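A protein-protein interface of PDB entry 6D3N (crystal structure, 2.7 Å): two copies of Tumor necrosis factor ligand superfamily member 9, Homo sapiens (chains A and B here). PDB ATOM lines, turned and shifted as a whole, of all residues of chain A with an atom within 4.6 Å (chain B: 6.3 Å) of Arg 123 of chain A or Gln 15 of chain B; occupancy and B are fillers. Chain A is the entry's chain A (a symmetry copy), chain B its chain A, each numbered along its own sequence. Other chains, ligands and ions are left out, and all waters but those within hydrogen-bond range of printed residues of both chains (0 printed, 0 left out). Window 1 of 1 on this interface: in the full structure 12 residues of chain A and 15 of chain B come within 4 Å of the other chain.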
ATOM      1  N   TYR A  62      21.609  -7.275   0.989  1.00  0.00           N
ATOM      2  CA  TYR A  62      20.998  -6.114   1.603  1.00  0.00           C
ATOM      3  C   TYR A  62      21.608  -4.867   1.023  1.00  0.00           C
ATOM      4  O   TYR A  62      22.808  -4.837   0.768  1.00  0.00           O
ATOM      5  CB  TYR A  62      21.272  -6.122   3.105  1.00  0.00           C
ATOM      6  CG  TYR A  62      20.435  -7.104   3.867  1.00  0.00           C
ATOM      7  CD1 TYR A  62      20.804  -8.433   3.947  1.00  0.00           C
ATOM      8  CD2 TYR A  62      19.258  -6.703   4.503  1.00  0.00           C
ATOM      9  CE1 TYR A  62      20.027  -9.347   4.644  1.00  0.00           C
ATOM     10  CE2 TYR A  62      18.477  -7.601   5.207  1.00  0.00           C
ATOM     11  CZ  TYR A  62      18.869  -8.924   5.277  1.00  0.00           C
ATOM     12  OH  TYR A  62      18.114  -9.830   5.972  1.00  0.00           O
ATOM     13  N   TYR A  63      20.796  -3.839   0.816  1.00  0.00           N
ATOM     14  CA  TYR A  63      21.325  -2.502   0.626  1.00  0.00           C
ATOM     15  C   TYR A  63      21.590  -1.932   2.007  1.00  0.00           C
ATOM     16  O   TYR A  63      20.680  -1.878   2.819  1.00  0.00           O
ATOM     17  CB  TYR A  63      20.342  -1.608  -0.118  1.00  0.00           C
ATOM     18  CG  TYR A  63      20.949  -0.266  -0.409  1.00  0.00           C
ATOM     19  CD1 TYR A  63      22.004  -0.154  -1.314  1.00  0.00           C
ATOM     20  CD2 TYR A  63      20.516   0.877   0.247  1.00  0.00           C
ATOM     21  CE1 TYR A  63      22.600   1.059  -1.573  1.00  0.00           C
ATOM     22  CE2 TYR A  63      21.100   2.103  -0.011  1.00  0.00           C
ATOM     23  CZ  TYR A  63      22.143   2.189  -0.923  1.00  0.00           C
ATOM     24  OH  TYR A  63      22.750   3.394  -1.189  1.00  0.00           O
ATOM     25  N   VAL A  64      22.826  -1.527   2.283  1.00  0.00           N
ATOM     26  CA  VAL A  64      23.191  -1.028   3.612  1.00  0.00           C
ATOM     27  C   VAL A  64      23.764   0.366   3.503  1.00  0.00           C
ATOM     28  O   VAL A  64      24.643   0.606   2.704  1.00  0.00           O
ATOM     29  CB  VAL A  64      24.253  -1.912   4.293  1.00  0.00           C
ATOM     30  CG1 VAL A  64      24.621  -1.355   5.671  1.00  0.00           C
ATOM     31  CG2 VAL A  64      23.756  -3.347   4.400  1.00  0.00           C
ATOM     32  N   ALA A  99      33.525  -3.784   5.796  1.00  0.00           N
ATOM     33  CA  ALA A  99      32.519  -3.899   4.731  1.00  0.00           C
ATOM     34  C   ALA A  99      32.097  -2.523   4.187  1.00  0.00           C
ATOM     35  O   ALA A  99      31.772  -2.377   3.006  1.00  0.00           O
ATOM     36  CB  ALA A  99      31.299  -4.661   5.242  1.00  0.00           C
ATOM     37  N   LEU A 100      32.095  -1.528   5.068  1.00  0.00           N
ATOM     38  CA  LEU A 100      31.661  -0.183   4.743  1.00  0.00           C
ATOM     39  C   LEU A 100      32.514   0.767   5.553  1.00  0.00           C
ATOM     40  O   LEU A 100      32.779   0.500   6.719  1.00  0.00           O
ATOM     41  CB  LEU A 100      30.193  -0.038   5.141  1.00  0.00           C
ATOM     42  CG  LEU A 100      29.317   0.937   4.371  1.00  0.00           C
ATOM     43  CD1 LEU A 100      29.196   0.503   2.926  1.00  0.00           C
ATOM     44  CD2 LEU A 100      27.939   1.027   5.017  1.00  0.00           C
ATOM     45  N   GLY A 122      26.428   4.173   0.944  1.00  0.00           N
ATOM     46  CA  GLY A 122      25.650   2.945   0.880  1.00  0.00           C
ATOM     47  C   GLY A 122      26.216   1.985  -0.139  1.00  0.00           C
ATOM     48  O   GLY A 122      26.811   2.415  -1.118  1.00  0.00           O
ATOM     49  N   ARG A 123      26.052   0.685   0.106  1.00  0.00           N
ATOM     50  CA  ARG A 123      26.259  -0.340  -0.917  1.00  0.00           C
ATOM     51  C   ARG A 123      25.592  -1.672  -0.611  1.00  0.00           C
ATOM     52  O   ARG A 123      25.125  -1.919   0.503  1.00  0.00           O
ATOM     53  CB  ARG A 123      27.743  -0.579  -1.164  1.00  0.00           C
ATOM     54  CG  ARG A 123      28.484  -1.221  -0.014  1.00  0.00           C
ATOM     55  CD  ARG A 123      29.942  -0.798  -0.025  1.00  0.00           C
ATOM     56  NE  ARG A 123      30.765  -1.569  -0.950  1.00  0.00           N
ATOM     57  CZ  ARG A 123      31.996  -1.229  -1.338  1.00  0.00           C
ATOM     58  NH1 ARG A 123      32.562  -0.081  -0.929  1.00  0.00           N
ATOM     59  NH2 ARG A 123      32.664  -2.043  -2.166  1.00  0.00           N
ATOM     60  N   LEU A 124      25.569  -2.518  -1.638  1.00  0.00           N
ATOM     61  CA  LEU A 124      24.993  -3.846  -1.562  1.00  0.00           C
ATOM     62  C   LEU A 124      25.948  -4.775  -0.832  1.00  0.00           C
ATOM     63  O   LEU A 124      27.137  -4.775  -1.115  1.00  0.00           O
ATOM     64  CB  LEU A 124      24.692  -4.367  -2.967  1.00  0.00           C
ATOM     65  CG  LEU A 124      23.537  -3.632  -3.657  1.00  0.00           C
ATOM     66  CD1 LEU A 124      23.532  -3.853  -5.159  1.00  0.00           C
ATOM     67  CD2 LEU A 124      22.196  -4.049  -3.066  1.00  0.00           C
ATOM     68  N   LEU A 125      25.419  -5.537   0.126  1.00  0.00           N
ATOM     69  CA  LEU A 125      26.192  -6.506   0.923  1.00  0.00           C
ATOM     70  C   LEU A 125      25.488  -7.858   0.965  1.00  0.00           C
ATOM     71  O   LEU A 125      24.271  -7.913   1.166  1.00  0.00           O
ATOM     72  CB  LEU A 125      26.338  -6.030   2.368  1.00  0.00           C
ATOM     73  CG  LEU A 125      27.215  -4.838   2.751  1.00  0.00           C
ATOM     74  CD1 LEU A 125      27.394  -4.828   4.268  1.00  0.00           C
ATOM     75  CD2 LEU A 125      28.573  -4.864   2.068  1.00  0.00           C
ATOM     76  N   PHE B  13      19.977  -7.471  -9.540  1.00  0.00           N
ATOM     77  CA  PHE B  13      20.863  -6.485  -8.962  1.00  0.00           C
ATOM     78  C   PHE B  13      22.278  -6.739  -9.436  1.00  0.00           C
ATOM     79  O   PHE B  13      22.577  -7.802  -9.961  1.00  0.00           O
ATOM     80  CB  PHE B  13      20.823  -6.566  -7.427  1.00  0.00           C
ATOM     81  CG  PHE B  13      21.359  -7.863  -6.866  1.00  0.00           C
ATOM     82  CD1 PHE B  13      20.491  -8.878  -6.473  1.00  0.00           C
ATOM     83  CD2 PHE B  13      22.740  -8.075  -6.729  1.00  0.00           C
ATOM     84  CE1 PHE B  13      20.982 -10.078  -5.966  1.00  0.00           C
ATOM     85  CE2 PHE B  13      23.231  -9.273  -6.227  1.00  0.00           C
ATOM     86  CZ  PHE B  13      22.350 -10.278  -5.845  1.00  0.00           C
ATOM     87  N   ALA B  14      23.155  -5.776  -9.194  1.00  0.00           N
ATOM     88  CA  ALA B  14      24.574  -5.933  -9.483  1.00  0.00           C
ATOM     89  C   ALA B  14      25.382  -4.863  -8.800  1.00  0.00           C
ATOM     90  O   ALA B  14      24.893  -3.783  -8.511  1.00  0.00           O
ATOM     91  CB  ALA B  14      24.830  -5.885 -10.979  1.00  0.00           C
ATOM     92  N   GLN B  15      26.640  -5.183  -8.567  1.00  0.00           N
ATOM     93  CA  GLN B  15      27.587  -4.247  -8.021  1.00  0.00           C
ATOM     94  C   GLN B  15      28.979  -4.546  -8.576  1.00  0.00           C
ATOM     95  O   GLN B  15      29.418  -5.684  -8.542  1.00  0.00           O
ATOM     96  CB  GLN B  15      27.560  -4.341  -6.511  1.00  0.00           C
ATOM     97  CG  GLN B  15      28.473  -3.341  -5.821  1.00  0.00           C
ATOM     98  CD  GLN B  15      27.994  -3.028  -4.426  1.00  0.00           C
ATOM     99  OE1 GLN B  15      27.103  -2.209  -4.247  1.00  0.00           O
ATOM    100  NE2 GLN B  15      28.566  -3.691  -3.438  1.00  0.00           N
ATOM    101  N   LEU B  16      29.647  -3.519  -9.097  1.00  0.00           N
ATOM    102  CA  LEU B  16      30.970  -3.638  -9.692  1.00  0.00           C
ATOM    103  C   LEU B  16      31.935  -2.700  -8.997  1.00  0.00           C
ATOM    104  O   LEU B  16      31.549  -1.654  -8.499  1.00  0.00           O
ATOM    105  CB  LEU B  16      30.923  -3.270 -11.167  1.00  0.00           C
ATOM    106  CG  LEU B  16      29.836  -3.921 -12.023  1.00  0.00           C
ATOM    107  CD1 LEU B  16      29.680  -3.141 -13.317  1.00  0.00           C
ATOM    108  CD2 LEU B  16      30.147  -5.385 -12.290  1.00  0.00           C
ATOM    109  N   VAL B  17      33.201  -3.076  -9.000  1.00  0.00           N
ATOM    110  CA  VAL B  17      34.269  -2.288  -8.417  1.00  0.00           C
ATOM    111  C   VAL B  17      35.254  -1.909  -9.542  1.00  0.00           C
ATOM    112  O   VAL B  17      35.524  -2.708 -10.452  1.00  0.00           O
ATOM    113  CB  VAL B  17      34.956  -3.106  -7.323  1.00  0.00           C
ATOM    114  CG1 VAL B  17      36.098  -2.321  -6.692  1.00  0.00           C
ATOM    115  CG2 VAL B  17      33.926  -3.555  -6.281  1.00  0.00           C
ATOM    116  N   TYR B  31      34.990  -4.815 -12.396  1.00  0.00           N
ATOM    117  CA  TYR B  31      34.952  -6.238 -12.116  1.00  0.00           C
ATOM    118  C   TYR B  31      33.891  -6.493 -11.063  1.00  0.00           C
ATOM    119  O   TYR B  31      33.691  -5.645 -10.202  1.00  0.00           O
ATOM    120  CB  TYR B  31      36.339  -6.720 -11.663  1.00  0.00           C
ATOM    121  CG  TYR B  31      36.767  -6.328 -10.269  1.00  0.00           C
ATOM    122  CD1 TYR B  31      37.495  -5.160 -10.026  1.00  0.00           C
ATOM    123  CD2 TYR B  31      36.509  -7.165  -9.196  1.00  0.00           C
ATOM    124  CE1 TYR B  31      37.916  -4.829  -8.737  1.00  0.00           C
ATOM    125  CE2 TYR B  31      36.909  -6.837  -7.906  1.00  0.00           C
ATOM    126  CZ  TYR B  31      37.611  -5.674  -7.682  1.00  0.00           C
ATOM    127  OH  TYR B  31      37.985  -5.392  -6.398  1.00  0.00           O
ATOM    128  N   SER B  32      33.215  -7.645 -11.133  1.00  0.00           N
ATOM    129  CA  SER B  32      32.217  -8.012 -10.119  1.00  0.00           C
ATOM    130  C   SER B  32      32.745  -7.932  -8.689  1.00  0.00           C
ATOM    131  O   SER B  32      33.890  -8.255  -8.419  1.00  0.00           O
ATOM    132  CB  SER B  32      31.668  -9.419 -10.346  1.00  0.00           C
ATOM    133  OG  SER B  32      30.477  -9.366 -11.089  1.00  0.00           O
ATOM    134  N   ASP B  33      31.882  -7.521  -7.771  1.00  0.00           N
ATOM    135  CA  ASP B  33      32.258  -7.402  -6.370  1.00  0.00           C
ATOM    136  C   ASP B  33      32.530  -8.809  -5.813  1.00  0.00           C
ATOM    137  O   ASP B  33      31.691  -9.695  -5.980  1.00  0.00           O
ATOM    138  CB  ASP B  33      31.147  -6.709  -5.568  1.00  0.00           C
ATOM    139  CG  ASP B  33      31.624  -6.202  -4.223  1.00  0.00           C
ATOM    140  OD1 ASP B  33      31.252  -5.066  -3.871  1.00  0.00           O
ATOM    141  OD2 ASP B  33      32.363  -6.921  -3.516  1.00  0.00           O
ATOM    142  N   LEU B  36      29.826 -10.355  -3.200  1.00  0.00           N
ATOM    143  CA  LEU B  36      28.552 -10.946  -3.632  1.00  0.00           C
ATOM    144  C   LEU B  36      28.706 -12.247  -4.420  1.00  0.00           C
ATOM    145  O   LEU B  36      29.812 -12.754  -4.615  1.00  0.00           O
ATOM    146  CB  LEU B  36      27.801  -9.945  -4.509  1.00  0.00           C
ATOM    147  CG  LEU B  36      27.508  -8.551  -3.945  1.00  0.00           C
ATOM    148  CD1 LEU B  36      26.923  -7.695  -5.049  1.00  0.00           C
ATOM    149  CD2 LEU B  36      26.553  -8.603  -2.761  1.00  0.00           C
ATOM    150  N   PHE B  65      23.391   3.601  -8.081  1.00  0.00           N
ATOM    151  CA  PHE B  65      24.272   4.439  -7.283  1.00  0.00           C
ATOM    152  C   PHE B  65      25.704   4.226  -7.680  1.00  0.00           C
ATOM    153  O   PHE B  65      26.070   3.156  -8.124  1.00  0.00           O
ATOM    154  CB  PHE B  65      24.109   4.145  -5.793  1.00  0.00           C
ATOM    155  CG  PHE B  65      24.296   2.700  -5.433  1.00  0.00           C
ATOM    156  CD1 PHE B  65      25.538   2.225  -5.026  1.00  0.00           C
ATOM    157  CD2 PHE B  65      23.224   1.810  -5.497  1.00  0.00           C
ATOM    158  CE1 PHE B  65      25.706   0.889  -4.690  1.00  0.00           C
ATOM    159  CE2 PHE B  65      23.387   0.475  -5.161  1.00  0.00           C
ATOM    160  CZ  PHE B  65      24.626   0.017  -4.753  1.00  0.00           C
ATOM    161  N   GLN B  67      29.915   5.778  -6.434  1.00  0.00           N
ATOM    162  CA  GLN B  67      30.685   6.135  -5.275  1.00  0.00           C
ATOM    163  C   GLN B  67      32.120   6.256  -5.764  1.00  0.00           C
ATOM    164  O   GLN B  67      32.561   5.471  -6.591  1.00  0.00           O
ATOM    165  CB  GLN B  67      30.540   4.991  -4.282  1.00  0.00           C
ATOM    166  CG  GLN B  67      31.327   5.084  -2.995  1.00  0.00           C
ATOM    167  CD  GLN B  67      31.200   3.823  -2.157  1.00  0.00           C
ATOM    168  OE1 GLN B  67      30.108   3.258  -2.019  1.00  0.00           O
ATOM    169  NE2 GLN B  67      32.322   3.365  -1.601  1.00  0.00           N
ATOM    170  N   PHE B 120      29.221  10.376  -3.312  1.00  0.00           N
ATOM    171  CA  PHE B 120      28.181   9.368  -3.470  1.00  0.00           C
ATOM    172  C   PHE B 120      26.968  10.016  -4.122  1.00  0.00           C
ATOM    173  O   PHE B 120      26.622  11.153  -3.810  1.00  0.00           O
ATOM    174  CB  PHE B 120      27.773   8.770  -2.128  1.00  0.00           C
ATOM    175  CG  PHE B 120      26.748   7.691  -2.252  1.00  0.00           C
ATOM    176  CD1 PHE B 120      27.134   6.367  -2.373  1.00  0.00           C
ATOM    177  CD2 PHE B 120      25.385   7.999  -2.289  1.00  0.00           C
ATOM    178  CE1 PHE B 120      26.192   5.361  -2.504  1.00  0.00           C
ATOM    179  CE2 PHE B 120      24.436   6.992  -2.431  1.00  0.00           C
ATOM    180  CZ  PHE B 120      24.843   5.670  -2.537  1.00  0.00           C
ATOM    181  N   GLY B 152      39.630  -0.196  -4.885  1.00  0.00           N
ATOM    182  CA  GLY B 152      38.446  -0.871  -4.334  1.00  0.00           C
ATOM    183  C   GLY B 152      37.296   0.018  -3.865  1.00  0.00           C
ATOM    184  O   GLY B 152      36.229  -0.493  -3.509  1.00  0.00           O
ATOM    185  N   ALA B 153      37.497   1.342  -3.887  1.00  0.00           N
ATOM    186  CA  ALA B 153      36.576   2.306  -3.280  1.00  0.00           C
ATOM    187  C   ALA B 153      35.661   3.037  -4.280  1.00  0.00           C
ATOM    188  O   ALA B 153      34.835   3.866  -3.873  1.00  0.00           O
ATOM    189  CB  ALA B 153      37.376   3.312  -2.471  1.00  0.00           C
ATOM    190  N   VAL B 155      32.732   2.292  -6.768  1.00  0.00           N
ATOM    191  CA  VAL B 155      31.729   1.250  -6.916  1.00  0.00           C
ATOM    192  C   VAL B 155      30.542   1.766  -7.715  1.00  0.00           C
ATOM    193  O   VAL B 155      30.141   2.913  -7.557  1.00  0.00           O
ATOM    194  CB  VAL B 155      31.255   0.819  -5.525  1.00  0.00           C
ATOM    195  CG1 VAL B 155      30.153  -0.229  -5.604  1.00  0.00           C
ATOM    196  CG2 VAL B 155      32.448   0.316  -4.729  1.00  0.00           C
ATOM    197  N   LEU B 156      30.004   0.918  -8.588  1.00  0.00           N
ATOM    198  CA  LEU B 156      28.734   1.169  -9.279  1.00  0.00           C
ATOM    199  C   LEU B 156      27.805   0.037  -8.885  1.00  0.00           C
ATOM    200  O   LEU B 156      28.128  -1.116  -9.108  1.00  0.00           O
ATOM    201  CB  LEU B 156      28.922   1.168 -10.788  1.00  0.00           C
ATOM    202  CG  LEU B 156      27.655   1.166 -11.661  1.00  0.00           C
ATOM    203  CD1 LEU B 156      26.816   2.419 -11.435  1.00  0.00           C
ATOM    204  CD2 LEU B 156      28.014   1.030 -13.145  1.00  0.00           C
ATOM    205  N   GLY B 157      26.658   0.361  -8.308  1.00  0.00           N
ATOM    206  CA  GLY B 157      25.715  -0.661  -7.919  1.00  0.00           C
ATOM    207  C   GLY B 157      24.315  -0.317  -8.335  1.00  0.00           C
ATOM    208  O   GLY B 157      24.006   0.843  -8.571  1.00  0.00           O
ATOM    209  N   LEU B 158      23.479  -1.342  -8.452  1.00  0.00           N
ATOM    210  CA  LEU B 158      22.079  -1.155  -8.789  1.00  0.00           C
ATOM    211  C   LEU B 158      21.239  -2.352  -8.422  1.00  0.00           C
ATOM    212  O   LEU B 158      21.744  -3.459  -8.317  1.00  0.00           O
ATOM    213  CB  LEU B 158      21.880  -0.842 -10.285  1.00  0.00           C
ATOM    214  CG  LEU B 158      21.933  -1.964 -11.328  1.00  0.00           C
ATOM    215  CD1 LEU B 158      21.690  -1.400 -12.708  1.00  0.00           C
ATOM    216  CD2 LEU B 158      23.266  -2.680 -11.292  1.00  0.00           C
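The backbone carbonyl oxygen (O) of Ala 14 of chain B is in hydrogen-bond range of the backbone NH (N) of Leu 158 of chain B (2.8 Å).
NE2 of Gln 15 of chain B is in hydrogen-bond range of OD1 of Asp 33 of chain B (3.0 Å).
The backbone NH (N) of Gly 157 of chain B lies within hydrogen-bond range of the backbone carbonyl oxygen (O) of Phe 65 of chain B, 2.9 Å away.
The backbone carbonyl oxygen (O) of Ala 153 of chain B sits at hydrogen-bond distance from the side-chain amide nitrogen (NE2) of Gln 67 of chain B (3.4 Å).
O of Leu 125 of chain A lies within hydrogen-bond range of N of Tyr 62 of chain A (2.7 Å).
The backbone NH of Val 64 of chain A sits at hydrogen-bond distance from the backbone carbonyl oxygen of Arg 123 of chain A, at 2.9 Å.
NE2 of Gln 15 of chain B sits at hydrogen-bond distance from O of Leu 124 of chain A (2.9 Å).
The side-chain carboxylate (OD1) of Asp 33 of chain B is in salt-bridge range of the guanidinium group (NH2) of Arg 123 of chain A, 3.7 Å away.
Ala 99 of chain A touches none of the printed residues of chain B.
Of the printed residues of chain B, Gly 122 of chain A touches Gln 67 and Phe 120.
Of the printed residues of chain A, Ala 14 of chain B touches Leu 124 (3.6 Å).
Of the printed residues of chain A, Asp 33 of chain B touches Arg 123 (3.7 Å).
Of the printed residues of chain A, Gln 67 of chain B touches Gly 122 (3.5 Å) and Arg 123 (3.5 Å).
Printed residues of chain A within 4 Å of Val 155 of chain B: Arg 123.
Gly 157 of chain B touches none of the printed residues of chain A.
The nearest printed residue of chain B that does not touch Leu 125 of chain A is Gln 15 of chain B (5.1 Å).
Tyr 63 of chain A touches Phe 65 of chain B.
Phe 120 of chain B touches Tyr 63 of chain A (CZ to OH, 3.4 Å).
Phe 120 of chain B touches Gly 122 of chain A.
CB of Arg 123 of chain A touches OE1 of Gln 15 of chain B (3.5 Å).
Arg 123 of chain A touches Gln 67 of chain B.
Arg 123 of chain A touches Val 155 of chain B.
O of Ala 14 of chain B touches CD1 of Leu 124 of chain A (3.6 Å).
Phe 65 of chain B touches Leu 124 of chain A (CZ to CG, 3.96 Å).
O of Leu 158 of chain B touches CD1 of Leu 124 of chain A, 3.7 Å away.
CD2 of Leu 36 of chain B touches C of Leu 125 of chain A (3.9 Å).
Of the 9 printed residues of chain A, 5 touch a printed residue of chain B.
Of the 18 printed residues of chain B, 9 touch a printed residue of chain A.
Hydrophobic or aromatic side chains of chain B within 4 Å of the printed part of chain A: Leu 36, Phe 65, Phe 120 and Val 155.
Among the printed residues, Asp or Glu carboxylates within 4 Å of a Lys or Arg side-chain nitrogen of the other chain: Arg 123 of chain A with Asp 33 of chain B (3.7 Å).
No position is printed for both chains.
Of the 13 pairs that touch across the chains among the printed residues, none has its exchanged pair printed and touching as well.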
